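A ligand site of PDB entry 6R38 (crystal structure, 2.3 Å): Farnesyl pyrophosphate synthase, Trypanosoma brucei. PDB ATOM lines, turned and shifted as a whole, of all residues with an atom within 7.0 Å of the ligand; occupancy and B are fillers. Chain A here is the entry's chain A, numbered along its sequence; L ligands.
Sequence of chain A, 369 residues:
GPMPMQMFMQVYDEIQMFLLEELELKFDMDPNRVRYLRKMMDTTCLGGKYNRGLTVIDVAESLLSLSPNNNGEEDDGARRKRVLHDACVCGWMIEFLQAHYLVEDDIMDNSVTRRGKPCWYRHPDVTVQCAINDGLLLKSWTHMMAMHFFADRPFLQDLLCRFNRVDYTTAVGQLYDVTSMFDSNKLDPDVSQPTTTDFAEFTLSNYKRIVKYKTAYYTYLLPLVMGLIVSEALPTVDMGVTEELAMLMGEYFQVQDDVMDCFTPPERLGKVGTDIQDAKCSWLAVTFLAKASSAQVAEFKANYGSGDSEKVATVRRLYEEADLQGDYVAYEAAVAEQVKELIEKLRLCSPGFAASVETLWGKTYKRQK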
ATOM      1  N   LYS A  49     -11.291 -15.580  -1.196  1.00  0.00           N
ATOM      2  CA  LYS A  49     -12.066 -15.640   0.050  1.00  0.00           C
ATOM      3  C   LYS A  49     -11.815 -14.428   0.964  1.00  0.00           C
ATOM      4  O   LYS A  49     -12.615 -14.193   1.883  1.00  0.00           O
ATOM      5  CB  LYS A  49     -11.870 -16.977   0.774  1.00  0.00           C
ATOM      6  CG  LYS A  49     -13.089 -17.414   1.588  1.00  0.00           C
ATOM      7  CD  LYS A  49     -12.792 -18.695   2.386  1.00  0.00           C
ATOM      8  CE  LYS A  49     -13.964 -19.153   3.207  1.00  0.00           C
ATOM      9  NZ  LYS A  49     -13.651 -20.409   3.932  1.00  0.00           N
ATOM     10  N   TYR A  50     -10.749 -13.648   0.691  1.00  0.00           N
ATOM     11  CA  TYR A  50     -10.336 -12.463   1.463  1.00  0.00           C
ATOM     12  C   TYR A  50     -10.002 -12.796   2.931  1.00  0.00           C
ATOM     13  O   TYR A  50     -10.145 -11.934   3.808  1.00  0.00           O
ATOM     14  CB  TYR A  50     -11.384 -11.333   1.350  1.00  0.00           C
ATOM     15  CG  TYR A  50     -11.906 -11.100  -0.067  1.00  0.00           C
ATOM     16  CD1 TYR A  50     -11.091 -10.573  -1.051  1.00  0.00           C
ATOM     17  CD2 TYR A  50     -13.225 -11.421  -0.398  1.00  0.00           C
ATOM     18  CE1 TYR A  50     -11.559 -10.370  -2.349  1.00  0.00           C
ATOM     19  CE2 TYR A  50     -13.709 -11.192  -1.692  1.00  0.00           C
ATOM     20  CZ  TYR A  50     -12.881 -10.664  -2.663  1.00  0.00           C
ATOM     21  OH  TYR A  50     -13.365 -10.467  -3.931  1.00  0.00           O
ATOM     22  N   ASN A  51      -9.501 -14.020   3.192  1.00  0.00           N
ATOM     23  CA  ASN A  51      -9.165 -14.429   4.554  1.00  0.00           C
ATOM     24  C   ASN A  51      -8.130 -13.530   5.212  1.00  0.00           C
ATOM     25  O   ASN A  51      -8.297 -13.195   6.386  1.00  0.00           O
ATOM     26  CB  ASN A  51      -8.751 -15.899   4.640  1.00  0.00           C
ATOM     27  CG  ASN A  51      -9.848 -16.897   4.350  1.00  0.00           C
ATOM     28  OD1 ASN A  51      -9.702 -17.767   3.479  1.00  0.00           O
ATOM     29  ND2 ASN A  51     -10.968 -16.798   5.058  1.00  0.00           N
ATOM     30  N   ARG A  52      -7.100 -13.086   4.462  1.00  0.00           N
ATOM     31  CA  ARG A  52      -6.060 -12.195   4.996  1.00  0.00           C
ATOM     32  C   ARG A  52      -6.628 -10.798   5.330  1.00  0.00           C
ATOM     33  O   ARG A  52      -6.399 -10.290   6.428  1.00  0.00           O
ATOM     34  CB  ARG A  52      -4.851 -12.093   4.045  1.00  0.00           C
ATOM     35  CG  ARG A  52      -4.021 -13.354   3.946  1.00  0.00           C
ATOM     36  CD  ARG A  52      -3.039 -13.228   2.809  1.00  0.00           C
ATOM     37  NE  ARG A  52      -2.363 -14.495   2.474  1.00  0.00           N
ATOM     38  CZ  ARG A  52      -2.885 -15.449   1.713  1.00  0.00           C
ATOM     39  NH1 ARG A  52      -4.132 -15.354   1.272  1.00  0.00           N
ATOM     40  NH2 ARG A  52      -2.186 -16.545   1.445  1.00  0.00           N
ATOM     41  N   GLY A  53      -7.391 -10.239   4.388  1.00  0.00           N
ATOM     42  CA  GLY A  53      -8.024  -8.927   4.504  1.00  0.00           C
ATOM     43  C   GLY A  53      -9.074  -8.865   5.586  1.00  0.00           C
ATOM     44  O   GLY A  53      -9.079  -7.932   6.383  1.00  0.00           O
ATOM     45  N   THR A  55      -9.258 -10.841   8.187  1.00  0.00           N
ATOM     46  CA  THR A  55      -8.585 -11.039   9.476  1.00  0.00           C
ATOM     47  C   THR A  55      -8.248  -9.682  10.114  1.00  0.00           C
ATOM     48  O   THR A  55      -8.421  -9.539  11.319  1.00  0.00           O
ATOM     49  CB  THR A  55      -7.378 -11.992   9.369  1.00  0.00           C
ATOM     50  OG1 THR A  55      -7.837 -13.278   9.006  1.00  0.00           O
ATOM     51  CG2 THR A  55      -6.607 -12.120  10.655  1.00  0.00           C
ATOM     52  N   GLU A  95      -4.351  -8.016   0.517  1.00  0.00           N
ATOM     53  CA  GLU A  95      -4.998  -8.636  -0.646  1.00  0.00           C
ATOM     54  C   GLU A  95      -4.296  -8.267  -1.946  1.00  0.00           C
ATOM     55  O   GLU A  95      -4.116  -9.138  -2.801  1.00  0.00           O
ATOM     56  CB  GLU A  95      -6.512  -8.342  -0.704  1.00  0.00           C
ATOM     57  CG  GLU A  95      -7.308  -9.023   0.410  1.00  0.00           C
ATOM     58  CD  GLU A  95      -7.248 -10.545   0.539  1.00  0.00           C
ATOM     59  OE1 GLU A  95      -7.221 -11.045   1.690  1.00  0.00           O
ATOM     60  OE2 GLU A  95      -7.235 -11.235  -0.501  1.00  0.00           O
ATOM     61  N   GLN A  98      -0.939 -10.115  -2.041  1.00  0.00           N
ATOM     62  CA  GLN A  98      -1.265 -11.478  -2.452  1.00  0.00           C
ATOM     63  C   GLN A  98      -1.490 -11.507  -3.989  1.00  0.00           C
ATOM     64  O   GLN A  98      -0.924 -12.354  -4.694  1.00  0.00           O
ATOM     65  CB  GLN A  98      -2.501 -11.996  -1.661  1.00  0.00           C
ATOM     66  CG  GLN A  98      -3.126 -13.309  -2.152  1.00  0.00           C
ATOM     67  CD  GLN A  98      -2.268 -14.557  -2.025  1.00  0.00           C
ATOM     68  OE1 GLN A  98      -1.079 -14.526  -1.731  1.00  0.00           O
ATOM     69  NE2 GLN A  98      -2.871 -15.692  -2.299  1.00  0.00           N
ATOM     70  N   TYR A 218       3.341 -13.505   5.876  1.00  0.00           N
ATOM     71  CA  TYR A 218       2.373 -12.630   5.210  1.00  0.00           C
ATOM     72  C   TYR A 218       0.887 -13.119   5.352  1.00  0.00           C
ATOM     73  O   TYR A 218      -0.024 -12.289   5.326  1.00  0.00           O
ATOM     74  CB  TYR A 218       2.769 -12.346   3.721  1.00  0.00           C
ATOM     75  CG  TYR A 218       2.190 -13.275   2.662  1.00  0.00           C
ATOM     76  CD1 TYR A 218       2.825 -14.480   2.353  1.00  0.00           C
ATOM     77  CD2 TYR A 218       1.057 -12.920   1.941  1.00  0.00           C
ATOM     78  CE1 TYR A 218       2.281 -15.355   1.407  1.00  0.00           C
ATOM     79  CE2 TYR A 218       0.535 -13.773   0.965  1.00  0.00           C
ATOM     80  CZ  TYR A 218       1.140 -14.990   0.717  1.00  0.00           C
ATOM     81  OH  TYR A 218       0.627 -15.860  -0.219  1.00  0.00           O
ATOM     82  N   THR A 219       0.661 -14.433   5.517  1.00  0.00           N
ATOM     83  CA  THR A 219      -0.691 -14.973   5.578  1.00  0.00           C
ATOM     84  C   THR A 219      -1.268 -14.931   6.995  1.00  0.00           C
ATOM     85  O   THR A 219      -2.443 -14.585   7.155  1.00  0.00           O
ATOM     86  CB  THR A 219      -0.725 -16.382   4.969  1.00  0.00           C
ATOM     87  OG1 THR A 219      -0.186 -16.313   3.666  1.00  0.00           O
ATOM     88  CG2 THR A 219      -2.126 -16.971   4.898  1.00  0.00           C
ATOM     89  N   TYR A 220      -0.474 -15.302   8.002  1.00  0.00           N
ATOM     90  CA  TYR A 220      -0.960 -15.376   9.376  1.00  0.00           C
ATOM     91  C   TYR A 220      -0.483 -14.231  10.251  1.00  0.00           C
ATOM     92  O   TYR A 220      -1.323 -13.656  10.949  1.00  0.00           O
ATOM     93  CB  TYR A 220      -0.642 -16.759  10.013  1.00  0.00           C
ATOM     94  CG  TYR A 220      -1.430 -17.868   9.332  1.00  0.00           C
ATOM     95  CD1 TYR A 220      -2.690 -18.242   9.792  1.00  0.00           C
ATOM     96  CD2 TYR A 220      -0.967 -18.441   8.146  1.00  0.00           C
ATOM     97  CE1 TYR A 220      -3.445 -19.202   9.130  1.00  0.00           C
ATOM     98  CE2 TYR A 220      -1.729 -19.385   7.458  1.00  0.00           C
ATOM     99  CZ  TYR A 220      -2.975 -19.759   7.945  1.00  0.00           C
ATOM    100  OH  TYR A 220      -3.743 -20.700   7.293  1.00  0.00           O
ATOM    101  N   PRO A 223      -1.644 -10.066   8.802  1.00  0.00           N
ATOM    102  CA  PRO A 223      -3.004  -9.594   9.085  1.00  0.00           C
ATOM    103  C   PRO A 223      -3.238  -9.287  10.554  1.00  0.00           C
ATOM    104  O   PRO A 223      -3.847  -8.257  10.855  1.00  0.00           O
ATOM    105  CB  PRO A 223      -3.878 -10.748   8.608  1.00  0.00           C
ATOM    106  CG  PRO A 223      -3.070 -11.429   7.591  1.00  0.00           C
ATOM    107  CD  PRO A 223      -1.688 -11.375   8.123  1.00  0.00           C
ATOM    108  N   PHE A 253      -1.676 -25.287   8.008  1.00  0.00           N
ATOM    109  CA  PHE A 253      -2.246 -24.989   6.718  1.00  0.00           C
ATOM    110  C   PHE A 253      -1.436 -25.614   5.576  1.00  0.00           C
ATOM    111  O   PHE A 253      -2.028 -26.190   4.665  1.00  0.00           O
ATOM    112  CB  PHE A 253      -2.364 -23.461   6.555  1.00  0.00           C
ATOM    113  CG  PHE A 253      -2.695 -22.996   5.161  1.00  0.00           C
ATOM    114  CD1 PHE A 253      -4.005 -23.000   4.707  1.00  0.00           C
ATOM    115  CD2 PHE A 253      -1.681 -22.608   4.288  1.00  0.00           C
ATOM    116  CE1 PHE A 253      -4.306 -22.668   3.400  1.00  0.00           C
ATOM    117  CE2 PHE A 253      -1.990 -22.235   2.984  1.00  0.00           C
ATOM    118  CZ  PHE A 253      -3.302 -22.256   2.559  1.00  0.00           C
ATOM    119  N   GLN A 256      -1.687 -29.558   5.347  1.00  0.00           N
ATOM    120  CA  GLN A 256      -2.978 -29.916   4.787  1.00  0.00           C
ATOM    121  C   GLN A 256      -2.996 -29.577   3.301  1.00  0.00           C
ATOM    122  O   GLN A 256      -3.469 -30.388   2.514  1.00  0.00           O
ATOM    123  CB  GLN A 256      -4.101 -29.216   5.566  1.00  0.00           C
ATOM    124  CG  GLN A 256      -5.500 -29.559   5.067  1.00  0.00           C
ATOM    125  CD  GLN A 256      -6.558 -28.717   5.717  1.00  0.00           C
ATOM    126  OE1 GLN A 256      -6.372 -27.538   6.028  1.00  0.00           O
ATOM    127  NE2 GLN A 256      -7.715 -29.318   5.901  1.00  0.00           N
ATOM    128  N   ASP A 257      -2.425 -28.427   2.921  1.00  0.00           N
ATOM    129  CA  ASP A 257      -2.336 -27.989   1.540  1.00  0.00           C
ATOM    130  C   ASP A 257      -1.511 -28.949   0.667  1.00  0.00           C
ATOM    131  O   ASP A 257      -1.873 -29.203  -0.479  1.00  0.00           O
ATOM    132  CB  ASP A 257      -1.723 -26.587   1.473  1.00  0.00           C
ATOM    133  CG  ASP A 257      -2.288 -25.775   0.339  1.00  0.00           C
ATOM    134  OD1 ASP A 257      -3.512 -25.545   0.333  1.00  0.00           O
ATOM    135  OD2 ASP A 257      -1.494 -25.371  -0.543  1.00  0.00           O
ATOM    136  N   THR A 359     -10.765 -17.343  15.743  1.00  0.00           N
ATOM    137  CA  THR A 359     -11.551 -17.304  14.518  1.00  0.00           C
ATOM    138  C   THR A 359     -10.625 -17.544  13.306  1.00  0.00           C
ATOM    139  O   THR A 359     -11.004 -18.327  12.421  1.00  0.00           O
ATOM    140  CB  THR A 359     -12.413 -16.035  14.465  1.00  0.00           C
ATOM    141  OG1 THR A 359     -13.579 -16.237  15.280  1.00  0.00           O
ATOM    142  CG2 THR A 359     -12.859 -15.671  13.059  1.00  0.00           C
ATOM    143  N   LEU A 360      -9.390 -16.945  13.310  1.00  0.00           N
ATOM    144  CA  LEU A 360      -8.388 -17.156  12.247  1.00  0.00           C
ATOM    145  C   LEU A 360      -8.044 -18.644  12.163  1.00  0.00           C
ATOM    146  O   LEU A 360      -8.023 -19.212  11.074  1.00  0.00           O
ATOM    147  CB  LEU A 360      -7.131 -16.284  12.453  1.00  0.00           C
ATOM    148  CG  LEU A 360      -5.954 -16.452  11.452  1.00  0.00           C
ATOM    149  CD1 LEU A 360      -6.371 -16.139  10.025  1.00  0.00           C
ATOM    150  CD2 LEU A 360      -4.779 -15.569  11.830  1.00  0.00           C
ATOM    151  N   TRP A 361      -7.863 -19.269  13.347  1.00  0.00           N
ATOM    152  CA  TRP A 361      -7.582 -20.692  13.506  1.00  0.00           C
ATOM    153  C   TRP A 361      -8.747 -21.585  13.034  1.00  0.00           C
ATOM    154  O   TRP A 361      -8.502 -22.593  12.374  1.00  0.00           O
ATOM    155  CB  TRP A 361      -7.214 -20.997  14.963  1.00  0.00           C
ATOM    156  CG  TRP A 361      -7.101 -22.454  15.275  1.00  0.00           C
ATOM    157  CD1 TRP A 361      -7.782 -23.140  16.242  1.00  0.00           C
ATOM    158  CD2 TRP A 361      -6.257 -23.410  14.621  1.00  0.00           C
ATOM    159  NE1 TRP A 361      -7.410 -24.465  16.243  1.00  0.00           N
ATOM    160  CE2 TRP A 361      -6.464 -24.651  15.262  1.00  0.00           C
ATOM    161  CE3 TRP A 361      -5.322 -23.332  13.588  1.00  0.00           C
ATOM    162  CZ2 TRP A 361      -5.763 -25.810  14.903  1.00  0.00           C
ATOM    163  CZ3 TRP A 361      -4.648 -24.479  13.205  1.00  0.00           C
ATOM    164  CH2 TRP A 361      -4.868 -25.696  13.864  1.00  0.00           C
ATOM    165  N   GLY A 362      -9.978 -21.209  13.362  1.00  0.00           N
ATOM    166  CA  GLY A 362     -11.169 -21.926  12.898  1.00  0.00           C
ATOM    167  C   GLY A 362     -11.274 -21.977  11.384  1.00  0.00           C
ATOM    168  O   GLY A 362     -11.683 -22.994  10.823  1.00  0.00           O
ATOM    169  N   LYS A 363     -10.845 -20.890  10.698  1.00  0.00           N
ATOM    170  CA  LYS A 363     -10.818 -20.798   9.238  1.00  0.00           C
ATOM    171  C   LYS A 363      -9.785 -21.748   8.613  1.00  0.00           C
ATOM    172  O   LYS A 363      -9.981 -22.196   7.479  1.00  0.00           O
ATOM    173  CB  LYS A 363     -10.534 -19.351   8.794  1.00  0.00           C
ATOM    174  CG  LYS A 363     -11.653 -18.380   9.124  1.00  0.00           C
ATOM    175  CD  LYS A 363     -11.390 -17.000   8.578  1.00  0.00           C
ATOM    176  CE  LYS A 363     -12.622 -16.162   8.702  1.00  0.00           C
ATOM    177  NZ  LYS A 363     -12.368 -14.913   9.467  1.00  0.00           N
ATOM    178  N   THR A 364      -8.683 -22.046   9.350  1.00  0.00           N
ATOM    179  CA  THR A 364      -7.588 -22.949   8.948  1.00  0.00           C
ATOM    180  C   THR A 364      -7.929 -24.402   9.265  1.00  0.00           C
ATOM    181  O   THR A 364      -7.703 -25.281   8.431  1.00  0.00           O
ATOM    182  CB  THR A 364      -6.285 -22.552   9.659  1.00  0.00           C
ATOM    183  OG1 THR A 364      -6.036 -21.160   9.482  1.00  0.00           O
ATOM    184  CG2 THR A 364      -5.086 -23.368   9.177  1.00  0.00           C
ATOM    185  N   TYR A 365      -8.438 -24.660  10.493  1.00  0.00           N
ATOM    186  CA  TYR A 365      -8.798 -25.985  11.015  1.00  0.00           C
ATOM    187  C   TYR A 365      -9.986 -26.622  10.248  1.00  0.00           C
ATOM    188  O   TYR A 365     -10.108 -27.842  10.261  1.00  0.00           O
ATOM    189  CB  TYR A 365      -9.058 -25.868  12.525  1.00  0.00           C
ATOM    190  CG  TYR A 365      -9.210 -27.172  13.247  1.00  0.00           C
ATOM    191  CD1 TYR A 365     -10.471 -27.640  13.628  1.00  0.00           C
ATOM    192  CD2 TYR A 365      -8.102 -27.932  13.613  1.00  0.00           C
ATOM    193  CE1 TYR A 365     -10.618 -28.820  14.350  1.00  0.00           C
ATOM    194  CE2 TYR A 365      -8.236 -29.123  14.332  1.00  0.00           C
ATOM    195  CZ  TYR A 365      -9.496 -29.560  14.701  1.00  0.00           C
ATOM    196  OH  TYR A 365      -9.646 -30.745  15.388  1.00  0.00           O
ATOM    197  N   LYS A 366     -10.783 -25.802   9.530  1.00  0.00           N
ATOM    198  CA  LYS A 366     -11.941 -26.142   8.687  1.00  0.00           C
ATOM    199  C   LYS A 366     -11.535 -27.069   7.521  1.00  0.00           C
ATOM    200  O   LYS A 366     -11.860 -26.828   6.354  1.00  0.00           O
ATOM    201  CB  LYS A 366     -12.570 -24.836   8.142  1.00  0.00           C
ATOM    202  CG  LYS A 366     -14.078 -24.873   7.996  1.00  0.00           C
ATOM    203  CD  LYS A 366     -14.628 -23.545   7.462  1.00  0.00           C
ATOM    204  CE  LYS A 366     -16.136 -23.468   7.482  1.00  0.00           C
ATOM    205  NZ  LYS A 366     -16.768 -24.330   6.443  1.00  0.00           N
HETATM  206  C1  LIG L   1      -7.234 -21.047   3.348  1.00  0.00           C
HETATM  207  C2  LIG L   1      -6.446 -19.961   3.240  1.00  0.00           C
HETATM  208  C3  LIG L   1      -5.855 -17.561   6.198  1.00  0.00           C
HETATM  209  C4  LIG L   1      -6.670 -18.220   7.137  1.00  0.00           C
HETATM  210  S1  LIG L   1      -8.002 -21.331   4.901  1.00  0.00           S
HETATM  211  C5  LIG L   1      -6.367 -19.230   4.562  1.00  0.00           C
HETATM  212  C6  LIG L   1      -7.196 -19.883   5.481  1.00  0.00           C
HETATM  213  C7  LIG L   1      -5.595 -19.651   2.035  1.00  0.00           C
HETATM  214  C8  LIG L   1      -5.801 -18.298   1.414  1.00  0.00           C
HETATM  215  C9  LIG L   1      -5.682 -18.056   4.897  1.00  0.00           C
HETATM  216 CL1  LIG L   1      -7.504 -22.148   2.016  1.00  0.00          CL
HETATM  217  C10 LIG L   1      -7.357 -19.393   6.787  1.00  0.00           C
HETATM  218  O1  LIG L   1      -5.094 -17.956   0.477  1.00  0.00           O
HETATM  219  O2  LIG L   1      -6.764 -17.541   1.943  1.00  0.00           O
HETATM  220 CL2  LIG L   1      -5.059 -16.070   6.625  1.00  0.00          CL
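OG1 of Thr 219 sits at hydrogen-bond distance from NH2 of Arg 52 (3.0 Å).
NH2 of Arg 52 lies within hydrogen-bond range of OH of Tyr 218, at 3.3 Å.
The side-chain carboxylate (OE1) of Glu 95 sits at hydrogen-bond distance from the backbone NH (N) of Arg 52, at 3.4 Å.
OG1 of Thr 55 sits at hydrogen-bond distance from O of Asn 51 (2.7 Å).
OG1 of Thr 364 is in hydrogen-bond range of O of Leu 360, 3.2 Å away.
OH of Tyr 220 lies within hydrogen-bond range of OG1 of Thr 364 (3.2 Å).
O of Lys 363 lies close to S1 of the ligand (3.4 Å).
O of Thr 219 touches CL2 of the ligand (3.1 Å).
Tyr 220 touches the ligand (OH to C4, 3.8 Å).
Phe 253 touches the ligand.
Leu 360 touches the ligand.
Thr 364 touches the ligand (OG1 to C10, 3.5 Å).
Hydrophobic or aromatic side chains within 4 Å of the ligand: Tyr 220, Phe 253 and Leu 360.
Of the 23 residues printed, 8 come within 4 Å of the ligand.
The nearest printed residue that does not touch the ligand is Gln 98 (4.2 Å).
O1 of the ligand lies within salt-bridge range of NH1 of Arg 52, 2.9 Å away.
The side-chain amide oxygen (OD1) of Asn 51 lies close to an oxygen (O2) of the ligand (3.3 Å).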
